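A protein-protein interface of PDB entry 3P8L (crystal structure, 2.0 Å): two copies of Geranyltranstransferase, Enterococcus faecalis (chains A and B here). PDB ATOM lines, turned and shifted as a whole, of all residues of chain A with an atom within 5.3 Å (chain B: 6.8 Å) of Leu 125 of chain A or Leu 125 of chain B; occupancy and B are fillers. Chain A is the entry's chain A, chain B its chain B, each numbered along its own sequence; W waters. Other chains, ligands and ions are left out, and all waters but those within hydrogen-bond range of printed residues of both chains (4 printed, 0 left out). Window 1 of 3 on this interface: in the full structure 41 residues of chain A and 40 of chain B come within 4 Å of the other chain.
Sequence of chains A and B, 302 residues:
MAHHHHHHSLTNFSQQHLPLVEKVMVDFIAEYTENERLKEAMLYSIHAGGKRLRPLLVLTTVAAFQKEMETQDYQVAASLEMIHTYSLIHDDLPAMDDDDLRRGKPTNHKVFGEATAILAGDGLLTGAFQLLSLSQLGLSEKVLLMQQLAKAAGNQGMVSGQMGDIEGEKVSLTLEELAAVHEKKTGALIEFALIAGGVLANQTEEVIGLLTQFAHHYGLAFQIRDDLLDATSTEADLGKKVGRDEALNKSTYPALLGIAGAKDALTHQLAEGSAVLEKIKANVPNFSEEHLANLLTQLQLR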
ATOM      1  N   MET A  82      22.815  -2.900  -5.325  1.00  0.00           N
ATOM      2  CA  MET A  82      21.416  -2.866  -4.872  1.00  0.00           C
ATOM      3  C   MET A  82      21.155  -1.719  -3.890  1.00  0.00           C
ATOM      4  O   MET A  82      20.131  -1.020  -4.014  1.00  0.00           O
ATOM      5  CB  MET A  82      20.936  -4.232  -4.328  1.00  0.00           C
ATOM      6  CG  MET A  82      20.838  -5.376  -5.426  1.00  0.00           C
ATOM      7  SD  MET A  82      20.545  -7.044  -4.739  1.00  0.00           S
ATOM      8  CE  MET A  82      18.846  -6.885  -4.181  1.00  0.00           C
ATOM      9  N   ILE A  83      22.088  -1.518  -2.949  1.00  0.00           N
ATOM     10  CA  ILE A  83      22.042  -0.414  -2.000  1.00  0.00           C
ATOM     11  C   ILE A  83      22.100   0.905  -2.768  1.00  0.00           C
ATOM     12  O   ILE A  83      21.272   1.800  -2.544  1.00  0.00           O
ATOM     13  CB  ILE A  83      23.213  -0.451  -0.960  1.00  0.00           C
ATOM     14  CG1 ILE A  83      23.108  -1.644  -0.017  1.00  0.00           C
ATOM     15  CG2 ILE A  83      23.302   0.868  -0.189  1.00  0.00           C
ATOM     16  CD1 ILE A  83      22.028  -1.548   1.033  1.00  0.00           C
ATOM     17  N   TYR A  86      18.837   1.471  -4.703  1.00  0.00           N
ATOM     18  CA  TYR A  86      17.785   1.884  -3.783  1.00  0.00           C
ATOM     19  C   TYR A  86      17.955   3.364  -3.441  1.00  0.00           C
ATOM     20  O   TYR A  86      16.981   4.113  -3.502  1.00  0.00           O
ATOM     21  CB  TYR A  86      17.668   0.987  -2.511  1.00  0.00           C
ATOM     22  CG  TYR A  86      17.929   1.699  -1.196  1.00  0.00           C
ATOM     23  CD1 TYR A  86      17.008   2.600  -0.674  1.00  0.00           C
ATOM     24  CD2 TYR A  86      19.102   1.480  -0.469  1.00  0.00           C
ATOM     25  CE1 TYR A  86      17.253   3.300   0.508  1.00  0.00           C
ATOM     26  CE2 TYR A  86      19.348   2.159   0.730  1.00  0.00           C
ATOM     27  CZ  TYR A  86      18.418   3.086   1.202  1.00  0.00           C
ATOM     28  OH  TYR A  86      18.611   3.758   2.388  1.00  0.00           O
ATOM     29  N   ALA A 120       9.828  -0.032  -3.938  1.00  0.00           N
ATOM     30  CA  ALA A 120      10.973  -0.579  -4.701  1.00  0.00           C
ATOM     31  C   ALA A 120      12.324  -0.294  -4.032  1.00  0.00           C
ATOM     32  O   ALA A 120      13.209  -1.191  -3.949  1.00  0.00           O
ATOM     33  CB  ALA A 120      10.977  -0.105  -6.142  1.00  0.00           C
ATOM     34  N   GLY A 121      12.481   0.932  -3.532  1.00  0.00           N
ATOM     35  CA  GLY A 121      13.671   1.282  -2.731  1.00  0.00           C
ATOM     36  C   GLY A 121      13.788   0.441  -1.459  1.00  0.00           C
ATOM     37  O   GLY A 121      14.869  -0.131  -1.169  1.00  0.00           O
ATOM     38  N   ASP A 122      12.686   0.325  -0.716  1.00  0.00           N
ATOM     39  CA  ASP A 122      12.643  -0.504   0.492  1.00  0.00           C
ATOM     40  C   ASP A 122      12.990  -1.969   0.196  1.00  0.00           C
ATOM     41  O   ASP A 122      13.656  -2.600   0.990  1.00  0.00           O
ATOM     42  CB  ASP A 122      11.271  -0.456   1.164  1.00  0.00           C
ATOM     43  CG  ASP A 122      10.936   0.911   1.735  1.00  0.00           C
ATOM     44  OD1 ASP A 122      11.827   1.790   1.816  1.00  0.00           O
ATOM     45  OD2 ASP A 122       9.770   1.091   2.131  1.00  0.00           O
ATOM     46  N   GLY A 123      12.526  -2.455  -0.949  1.00  0.00           N
ATOM     47  CA  GLY A 123      12.702  -3.823  -1.368  1.00  0.00           C
ATOM     48  C   GLY A 123      14.139  -4.080  -1.812  1.00  0.00           C
ATOM     49  O   GLY A 123      14.721  -5.127  -1.503  1.00  0.00           O
ATOM     50  N   LEU A 124      14.725  -3.099  -2.493  1.00  0.00           N
ATOM     51  CA  LEU A 124      16.100  -3.189  -2.890  1.00  0.00           C
ATOM     52  C   LEU A 124      17.061  -3.110  -1.705  1.00  0.00           C
ATOM     53  O   LEU A 124      18.033  -3.866  -1.671  1.00  0.00           O
ATOM     54  CB  LEU A 124      16.442  -2.166  -3.976  1.00  0.00           C
ATOM     55  CG  LEU A 124      16.017  -2.604  -5.396  1.00  0.00           C
ATOM     56  CD1 LEU A 124      15.973  -1.374  -6.268  1.00  0.00           C
ATOM     57  CD2 LEU A 124      16.961  -3.656  -5.994  1.00  0.00           C
ATOM     58  N   LEU A 125      16.803  -2.177  -0.776  1.00  0.00           N
ATOM     59  CA  LEU A 125      17.523  -2.094   0.497  1.00  0.00           C
ATOM     60  C   LEU A 125      17.495  -3.435   1.266  1.00  0.00           C
ATOM     61  O   LEU A 125      18.557  -3.954   1.619  1.00  0.00           O
ATOM     62  CB  LEU A 125      17.002  -0.946   1.385  1.00  0.00           C
ATOM     63  CG  LEU A 125      17.567  -0.778   2.813  1.00  0.00           C
ATOM     64  CD1 LEU A 125      19.084  -0.791   2.845  1.00  0.00           C
ATOM     65  CD2 LEU A 125      17.106   0.554   3.421  1.00  0.00           C
ATOM     66  N   THR A 126      16.302  -3.991   1.508  1.00  0.00           N
ATOM     67  CA  THR A 126      16.172  -5.260   2.236  1.00  0.00           C
ATOM     68  C   THR A 126      16.811  -6.400   1.432  1.00  0.00           C
ATOM     69  O   THR A 126      17.479  -7.296   1.994  1.00  0.00           O
ATOM     70  CB  THR A 126      14.685  -5.613   2.537  1.00  0.00           C
ATOM     71  OG1 THR A 126      14.026  -4.476   3.105  1.00  0.00           O
ATOM     72  CG2 THR A 126      14.583  -6.762   3.536  1.00  0.00           C
ATOM     73  N   GLY A 127      16.630  -6.336   0.118  1.00  0.00           N
ATOM     74  CA  GLY A 127      17.190  -7.306  -0.827  1.00  0.00           C
ATOM     75  C   GLY A 127      18.702  -7.389  -0.800  1.00  0.00           C
ATOM     76  O   GLY A 127      19.265  -8.461  -0.909  1.00  0.00           O
ATOM     77  N   ALA A 128      19.357  -6.243  -0.689  1.00  0.00           N
ATOM     78  CA  ALA A 128      20.815  -6.210  -0.587  1.00  0.00           C
ATOM     79  C   ALA A 128      21.321  -7.045   0.605  1.00  0.00           C
ATOM     80  O   ALA A 128      22.266  -7.844   0.463  1.00  0.00           O
ATOM     81  CB  ALA A 128      21.265  -4.797  -0.462  1.00  0.00           C
ATOM     82  N   PHE A 129      20.676  -6.868   1.762  1.00  0.00           N
ATOM     83  CA  PHE A 129      20.980  -7.655   2.955  1.00  0.00           C
ATOM     84  C   PHE A 129      20.554  -9.100   2.779  1.00  0.00           C
ATOM     85  O   PHE A 129      21.277  -9.993   3.204  1.00  0.00           O
ATOM     86  CB  PHE A 129      20.428  -7.009   4.240  1.00  0.00           C
ATOM     87  CG  PHE A 129      21.197  -5.776   4.631  1.00  0.00           C
ATOM     88  CD1 PHE A 129      22.451  -5.881   5.228  1.00  0.00           C
ATOM     89  CD2 PHE A 129      20.730  -4.527   4.303  1.00  0.00           C
ATOM     90  CE1 PHE A 129      23.187  -4.760   5.541  1.00  0.00           C
ATOM     91  CE2 PHE A 129      21.461  -3.385   4.614  1.00  0.00           C
ATOM     92  CZ  PHE A 129      22.688  -3.501   5.225  1.00  0.00           C
ATOM     93  N   MET B  42      13.890   9.384  14.170  1.00  0.00           N
ATOM     94  CA  MET B  42      13.729   7.962  14.462  1.00  0.00           C
ATOM     95  C   MET B  42      13.262   7.759  15.907  1.00  0.00           C
ATOM     96  O   MET B  42      12.406   6.896  16.168  1.00  0.00           O
ATOM     97  CB  MET B  42      15.003   7.172  14.125  1.00  0.00           C
ATOM     98  CG  MET B  42      15.355   7.130  12.624  1.00  0.00           C
ATOM     99  SD  MET B  42      16.879   6.271  12.112  1.00  0.00           S
ATOM    100  CE  MET B  42      18.072   7.194  13.069  1.00  0.00           C
ATOM    101  N   SER B  79      15.403  -5.363  17.050  1.00  0.00           N
ATOM    102  CA  SER B  79      15.604  -5.320  15.600  1.00  0.00           C
ATOM    103  C   SER B  79      14.260  -5.495  14.905  1.00  0.00           C
ATOM    104  O   SER B  79      13.908  -4.718  14.003  1.00  0.00           O
ATOM    105  CB  SER B  79      16.574  -6.425  15.151  1.00  0.00           C
ATOM    106  OG  SER B  79      17.904  -6.100  15.513  1.00  0.00           O
ATOM    107  N   MET B  82      12.163  -2.371  15.292  1.00  0.00           N
ATOM    108  CA  MET B  82      12.693  -1.322  14.415  1.00  0.00           C
ATOM    109  C   MET B  82      12.181  -1.507  12.980  1.00  0.00           C
ATOM    110  O   MET B  82      11.844  -0.519  12.326  1.00  0.00           O
ATOM    111  CB  MET B  82      14.234  -1.260  14.450  1.00  0.00           C
ATOM    112  CG  MET B  82      14.857  -0.719  15.765  1.00  0.00           C
ATOM    113  SD  MET B  82      16.635  -1.175  15.923  1.00  0.00           S
ATOM    114  CE  MET B  82      17.364   0.005  14.886  1.00  0.00           C
ATOM    115  N   ILE B  83      12.110  -2.763  12.506  1.00  0.00           N
ATOM    116  CA  ILE B  83      11.458  -3.068  11.221  1.00  0.00           C
ATOM    117  C   ILE B  83       9.995  -2.612  11.218  1.00  0.00           C
ATOM    118  O   ILE B  83       9.585  -1.849  10.331  1.00  0.00           O
ATOM    119  CB  ILE B  83      11.576  -4.576  10.848  1.00  0.00           C
ATOM    120  CG1 ILE B  83      13.047  -4.966  10.717  1.00  0.00           C
ATOM    121  CG2 ILE B  83      10.809  -4.910   9.574  1.00  0.00           C
ATOM    122  CD1 ILE B  83      13.713  -4.592   9.397  1.00  0.00           C
ATOM    123  N   TYR B  86       9.791   1.303  11.108  1.00  0.00           N
ATOM    124  CA  TYR B  86      10.061   1.846   9.780  1.00  0.00           C
ATOM    125  C   TYR B  86       8.865   1.708   8.850  1.00  0.00           C
ATOM    126  O   TYR B  86       8.493   2.689   8.190  1.00  0.00           O
ATOM    127  CB  TYR B  86      11.358   1.281   9.147  1.00  0.00           C
ATOM    128  CG  TYR B  86      11.173   0.494   7.857  1.00  0.00           C
ATOM    129  CD1 TYR B  86      10.992   1.141   6.628  1.00  0.00           C
ATOM    130  CD2 TYR B  86      11.186  -0.893   7.868  1.00  0.00           C
ATOM    131  CE1 TYR B  86      10.804   0.403   5.447  1.00  0.00           C
ATOM    132  CE2 TYR B  86      11.032  -1.639   6.691  1.00  0.00           C
ATOM    133  CZ  TYR B  86      10.837  -0.986   5.496  1.00  0.00           C
ATOM    134  OH  TYR B  86      10.653  -1.717   4.354  1.00  0.00           O
ATOM    135  N   HIS B  90       6.838   4.793   6.655  1.00  0.00           N
ATOM    136  CA  HIS B  90       6.681   4.828   5.215  1.00  0.00           C
ATOM    137  C   HIS B  90       5.203   4.687   4.817  1.00  0.00           C
ATOM    138  O   HIS B  90       4.760   5.372   3.911  1.00  0.00           O
ATOM    139  CB  HIS B  90       7.556   3.756   4.536  1.00  0.00           C
ATOM    140  CG  HIS B  90       8.998   4.154   4.393  1.00  0.00           C
ATOM    141  ND1 HIS B  90       9.893   3.443   3.620  1.00  0.00           N
ATOM    142  CD2 HIS B  90       9.697   5.190   4.917  1.00  0.00           C
ATOM    143  CE1 HIS B  90      11.078   4.024   3.675  1.00  0.00           C
ATOM    144  NE2 HIS B  90      10.990   5.082   4.458  1.00  0.00           N
ATOM    145  N   LEU B 119      13.858   9.087   5.101  1.00  0.00           N
ATOM    146  CA  LEU B 119      15.187   8.779   5.624  1.00  0.00           C
ATOM    147  C   LEU B 119      15.167   8.103   6.986  1.00  0.00           C
ATOM    148  O   LEU B 119      15.946   7.187   7.215  1.00  0.00           O
ATOM    149  CB  LEU B 119      16.092  10.023   5.641  1.00  0.00           C
ATOM    150  CG  LEU B 119      16.417  10.582   4.243  1.00  0.00           C
ATOM    151  CD1 LEU B 119      17.269  11.848   4.340  1.00  0.00           C
ATOM    152  CD2 LEU B 119      17.077   9.566   3.335  1.00  0.00           C
ATOM    153  N   ALA B 120      14.256   8.499   7.874  1.00  0.00           N
ATOM    154  CA  ALA B 120      14.128   7.836   9.170  1.00  0.00           C
ATOM    155  C   ALA B 120      13.716   6.372   9.004  1.00  0.00           C
ATOM    156  O   ALA B 120      14.265   5.493   9.661  1.00  0.00           O
ATOM    157  CB  ALA B 120      13.149   8.579  10.073  1.00  0.00           C
ATOM    158  N   GLY B 121      12.771   6.128   8.099  1.00  0.00           N
ATOM    159  CA  GLY B 121      12.357   4.774   7.752  1.00  0.00           C
ATOM    160  C   GLY B 121      13.523   3.990   7.176  1.00  0.00           C
ATOM    161  O   GLY B 121      13.814   2.888   7.641  1.00  0.00           O
ATOM    162  N   ASP B 122      14.209   4.570   6.186  1.00  0.00           N
ATOM    163  CA  ASP B 122      15.436   3.950   5.638  1.00  0.00           C
ATOM    164  C   ASP B 122      16.493   3.655   6.714  1.00  0.00           C
ATOM    165  O   ASP B 122      17.096   2.554   6.735  1.00  0.00           O
ATOM    166  CB  ASP B 122      16.029   4.837   4.535  1.00  0.00           C
ATOM    167  CG  ASP B 122      15.153   4.895   3.299  1.00  0.00           C
ATOM    168  OD1 ASP B 122      14.157   4.137   3.253  1.00  0.00           O
ATOM    169  OD2 ASP B 122      15.458   5.685   2.375  1.00  0.00           O
ATOM    170  N   GLY B 123      16.716   4.639   7.594  1.00  0.00           N
ATOM    171  CA  GLY B 123      17.646   4.511   8.715  1.00  0.00           C
ATOM    172  C   GLY B 123      17.279   3.403   9.699  1.00  0.00           C
ATOM    173  O   GLY B 123      18.130   2.593  10.107  1.00  0.00           O
ATOM    174  N   LEU B 124      16.004   3.337  10.065  1.00  0.00           N
ATOM    175  CA  LEU B 124      15.509   2.237  10.922  1.00  0.00           C
ATOM    176  C   LEU B 124      15.582   0.832  10.315  1.00  0.00           C
ATOM    177  O   LEU B 124      15.875  -0.131  11.020  1.00  0.00           O
ATOM    178  CB  LEU B 124      14.082   2.523  11.386  1.00  0.00           C
ATOM    179  CG  LEU B 124      13.995   3.508  12.560  1.00  0.00           C
ATOM    180  CD1 LEU B 124      12.596   4.114  12.635  1.00  0.00           C
ATOM    181  CD2 LEU B 124      14.323   2.797  13.856  1.00  0.00           C
ATOM    182  N   LEU B 125      15.302   0.721   9.013  1.00  0.00           N
ATOM    183  CA  LEU B 125      15.399  -0.555   8.318  1.00  0.00           C
ATOM    184  C   LEU B 125      16.858  -1.017   8.309  1.00  0.00           C
ATOM    185  O   LEU B 125      17.146  -2.160   8.677  1.00  0.00           O
ATOM    186  CB  LEU B 125      14.832  -0.466   6.884  1.00  0.00           C
ATOM    187  CG  LEU B 125      15.064  -1.610   5.876  1.00  0.00           C
ATOM    188  CD1 LEU B 125      14.679  -2.956   6.431  1.00  0.00           C
ATOM    189  CD2 LEU B 125      14.294  -1.360   4.563  1.00  0.00           C
ATOM    190  N   THR B 126      17.758  -0.135   7.898  1.00  0.00           N
ATOM    191  CA  THR B 126      19.175  -0.475   7.896  1.00  0.00           C
ATOM    192  C   THR B 126      19.628  -0.742   9.327  1.00  0.00           C
ATOM    193  O   THR B 126      20.326  -1.723   9.566  1.00  0.00           O
ATOM    194  CB  THR B 126      20.051   0.603   7.231  1.00  0.00           C
ATOM    195  OG1 THR B 126      19.461   0.981   5.987  1.00  0.00           O
ATOM    196  CG2 THR B 126      21.472   0.045   6.932  1.00  0.00           C
ATOM    197  N   GLY B 127      19.199   0.113  10.259  1.00  0.00           N
ATOM    198  CA  GLY B 127      19.502  -0.031  11.698  1.00  0.00           C
ATOM    199  C   GLY B 127      19.161  -1.399  12.275  1.00  0.00           C
ATOM    200  O   GLY B 127      19.924  -1.951  13.061  1.00  0.00           O
ATOM    201  N   ALA B 128      18.008  -1.943  11.895  1.00  0.00           N
ATOM    202  CA  ALA B 128      17.603  -3.279  12.355  1.00  0.00           C
ATOM    203  C   ALA B 128      18.571  -4.372  11.938  1.00  0.00           C
ATOM    204  O   ALA B 128      18.877  -5.285  12.738  1.00  0.00           O
ATOM    205  CB  ALA B 128      16.217  -3.606  11.841  1.00  0.00           C
ATOM    206  N   PHE B 129      19.050  -4.299  10.691  1.00  0.00           N
ATOM    207  CA  PHE B 129      20.051  -5.273  10.236  1.00  0.00           C
ATOM    208  C   PHE B 129      21.404  -5.060  10.891  1.00  0.00           C
ATOM    209  O   PHE B 129      22.083  -6.030  11.209  1.00  0.00           O
ATOM    210  CB  PHE B 129      20.136  -5.362   8.695  1.00  0.00           C
ATOM    211  CG  PHE B 129      18.952  -6.036   8.106  1.00  0.00           C
ATOM    212  CD1 PHE B 129      18.869  -7.425   8.093  1.00  0.00           C
ATOM    213  CD2 PHE B 129      17.864  -5.292   7.671  1.00  0.00           C
ATOM    214  CE1 PHE B 129      17.740  -8.059   7.604  1.00  0.00           C
ATOM    215  CE2 PHE B 129      16.740  -5.926   7.183  1.00  0.00           C
ATOM    216  CZ  PHE B 129      16.673  -7.307   7.159  1.00  0.00           C
ATOM    217  N   GLN B 130      21.773  -3.800  11.104  1.00  0.00           N
ATOM    218  CA  GLN B 130      23.028  -3.481  11.783  1.00  0.00           C
ATOM    219  C   GLN B 130      23.050  -4.056  13.200  1.00  0.00           C
ATOM    220  O   GLN B 130      23.989  -4.768  13.566  1.00  0.00           O
ATOM    221  CB  GLN B 130      23.302  -1.976  11.813  1.00  0.00           C
ATOM    222  CG  GLN B 130      24.743  -1.680  12.269  1.00  0.00           C
ATOM    223  CD  GLN B 130      25.161  -0.224  12.157  1.00  0.00           C
ATOM    224  OE1 GLN B 130      26.354   0.079  12.078  1.00  0.00           O
ATOM    225  NE2 GLN B 130      24.200   0.676  12.163  1.00  0.00           N
ATOM    226  N   LEU B 149      14.941 -12.547   8.826  1.00  0.00           N
ATOM    227  CA  LEU B 149      14.417 -11.195   8.957  1.00  0.00           C
ATOM    228  C   LEU B 149      14.308 -10.557   7.573  1.00  0.00           C
ATOM    229  O   LEU B 149      13.310  -9.908   7.281  1.00  0.00           O
ATOM    230  CB  LEU B 149      15.269 -10.324   9.892  1.00  0.00           C
ATOM    231  CG  LEU B 149      14.661  -8.953  10.217  1.00  0.00           C
ATOM    232  CD1 LEU B 149      13.264  -9.096  10.899  1.00  0.00           C
ATOM    233  CD2 LEU B 149      15.601  -8.100  11.053  1.00  0.00           C
ATOM    234  N   ALA B 153      10.808  -9.340   6.056  1.00  0.00           N
ATOM    235  CA  ALA B 153      10.600  -7.898   5.829  1.00  0.00           C
ATOM    236  C   ALA B 153      10.651  -7.439   4.373  1.00  0.00           C
ATOM    237  O   ALA B 153      10.167  -6.352   4.054  1.00  0.00           O
ATOM    238  CB  ALA B 153      11.590  -7.094   6.630  1.00  0.00           C
ATOM    239  N   MET B 158       6.963  -8.614   3.535  1.00  0.00           N
ATOM    240  CA  MET B 158       6.203  -7.393   3.870  1.00  0.00           C
ATOM    241  C   MET B 158       6.082  -6.356   2.724  1.00  0.00           C
ATOM    242  O   MET B 158       4.996  -5.789   2.502  1.00  0.00           O
ATOM    243  CB  MET B 158       6.792  -6.770   5.159  1.00  0.00           C
ATOM    244  CG  MET B 158       5.985  -5.582   5.779  1.00  0.00           C
ATOM    245  SD  MET B 158       6.780  -4.710   7.151  1.00  0.00           S
ATOM    246  CE  MET B 158       8.111  -3.939   6.285  1.00  0.00           C
ATOM    247  N   VAL B 159       7.180  -6.114   2.009  1.00  0.00           N
ATOM    248  CA  VAL B 159       7.201  -5.131   0.907  1.00  0.00           C
ATOM    249  C   VAL B 159       6.304  -5.580  -0.263  1.00  0.00           C
ATOM    250  O   VAL B 159       5.568  -4.755  -0.842  1.00  0.00           O
ATOM    251  CB  VAL B 159       8.655  -4.719   0.451  1.00  0.00           C
ATOM    252  CG1 VAL B 159       8.622  -3.661  -0.620  1.00  0.00           C
ATOM    253  CG2 VAL B 159       9.489  -4.181   1.635  1.00  0.00           C
HETATM  254  O   HOH W   1      11.624  -3.969   4.394  1.00  0.00           O
HETATM  255  O   HOH W   2       8.207  -0.678   3.385  1.00  0.00           O
HETATM  256  O   HOH W   3      18.279   6.355   1.823  1.00  0.00           O
HETATM  257  O   HOH W   4      20.456   2.508   3.855  1.00  0.00           O
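Water W1 lies within hydrogen-bond range of the side-chain hydroxyl of Tyr 86 of chain B (2.5 Å), the side-chain hydroxyl of Thr 126 of chain A (2.8 Å) and the backbone carbonyl oxygen of Ala 153 of chain B (2.8 Å). Water W4 lies within hydrogen-bond range of the side-chain hydroxyl (OH) of Tyr 86 of chain A (2.7 Å) and the side-chain hydroxyl (OG1) of Thr 126 of chain B (2.8 Å). Water W2 bridges the side-chain carboxylate of Asp 122 of chain A (2.7 Å) and the side-chain hydroxyl of Tyr 86 of chain B (2.8 Å). Water W3 bridges OH of Tyr 86 of chain A (2.7 Å) and OD2 of Asp 122 of chain B (3.0 Å).
The side-chain carboxylate (OD2) of Asp 122 of chain A sits at hydrogen-bond distance from a ring nitrogen (ND1) of His 90 of chain B, at 2.8 Å.
Leu 125 of chain A touches three residues of chain B. Of the printed residues of chain B, Thr 126 of chain A touches Leu 125. Of the printed residues of chain A, Tyr 86 of chain B touches Asp 122 (3.5 Å). Printed residues of chain A within 4 Å of His 90 of chain B: Asp 122. Of chain A, only Asp 122, Leu 125 and Thr 126 come within 4 Å of Leu 125 of chain B. Of the printed residues of chain A, Thr 126 of chain B touches Leu 125.
The backbone carbonyl oxygen (O) of Asp 122 of chain B is in hydrogen-bond range of the side-chain hydroxyl (OG1) of Thr 126 of chain B (2.9 Å). The side-chain hydroxyl (OG1) of Thr 126 of chain A lies within hydrogen-bond range of the backbone carbonyl oxygen (O) of Asp 122 of chain A (2.9 Å).
Asp 122 of chain B touches its own counterpart, Asp 122 of chain A. Asp 122 of chain A touches Leu 125 of chain B, and with the chains exchanged Leu 125 of chain A touches Asp 122 of chain B. Leu 125 of chain A touches its own counterpart, Leu 125 of chain B. Leu 125 of chain A touches Thr 126 of chain B, and with the chains exchanged Thr 126 of chain A touches Leu 125 of chain B. Positions printed for both chains: 82, 83, 86, 120, 121, 122, 123, 124, 125, 126, 127, 128 and 129.
Among the printed residues, pairs that only touch across the chains: Tyr 86 of chain A with Asp 122 of chain B (3.5 Å), Asp 122 of chain A with Tyr 86 of chain B (3.5 Å), Asp 122 of chain A with Asp 122 of chain B (3.6 Å), Asp 122 of chain A with Leu 125 of chain B (3.8 Å), Leu 125 of chain A with Asp 122 of chain B (3.9 Å), Leu 125 of chain A with Leu 125 of chain B (3.6 Å), Leu 125 of chain A with Thr 126 of chain B (3.5 Å) and Thr 126 of chain A with Leu 125 of chain B (3.5 Å).
Hydrophobic or aromatic side chains of chain A that line the printed part of chain B: Tyr 86 and Leu 125. Of the 22 printed residues of chain B, 5 touch a printed residue of chain A. Hydrophobic or aromatic side chains of chain B that line the printed part of chain A: Tyr 86, His 90 and Leu 125. Among the printed residues, no Asp or Glu carboxylate lies within 4 Å of a Lys or Arg side-chain nitrogen of the other chain.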
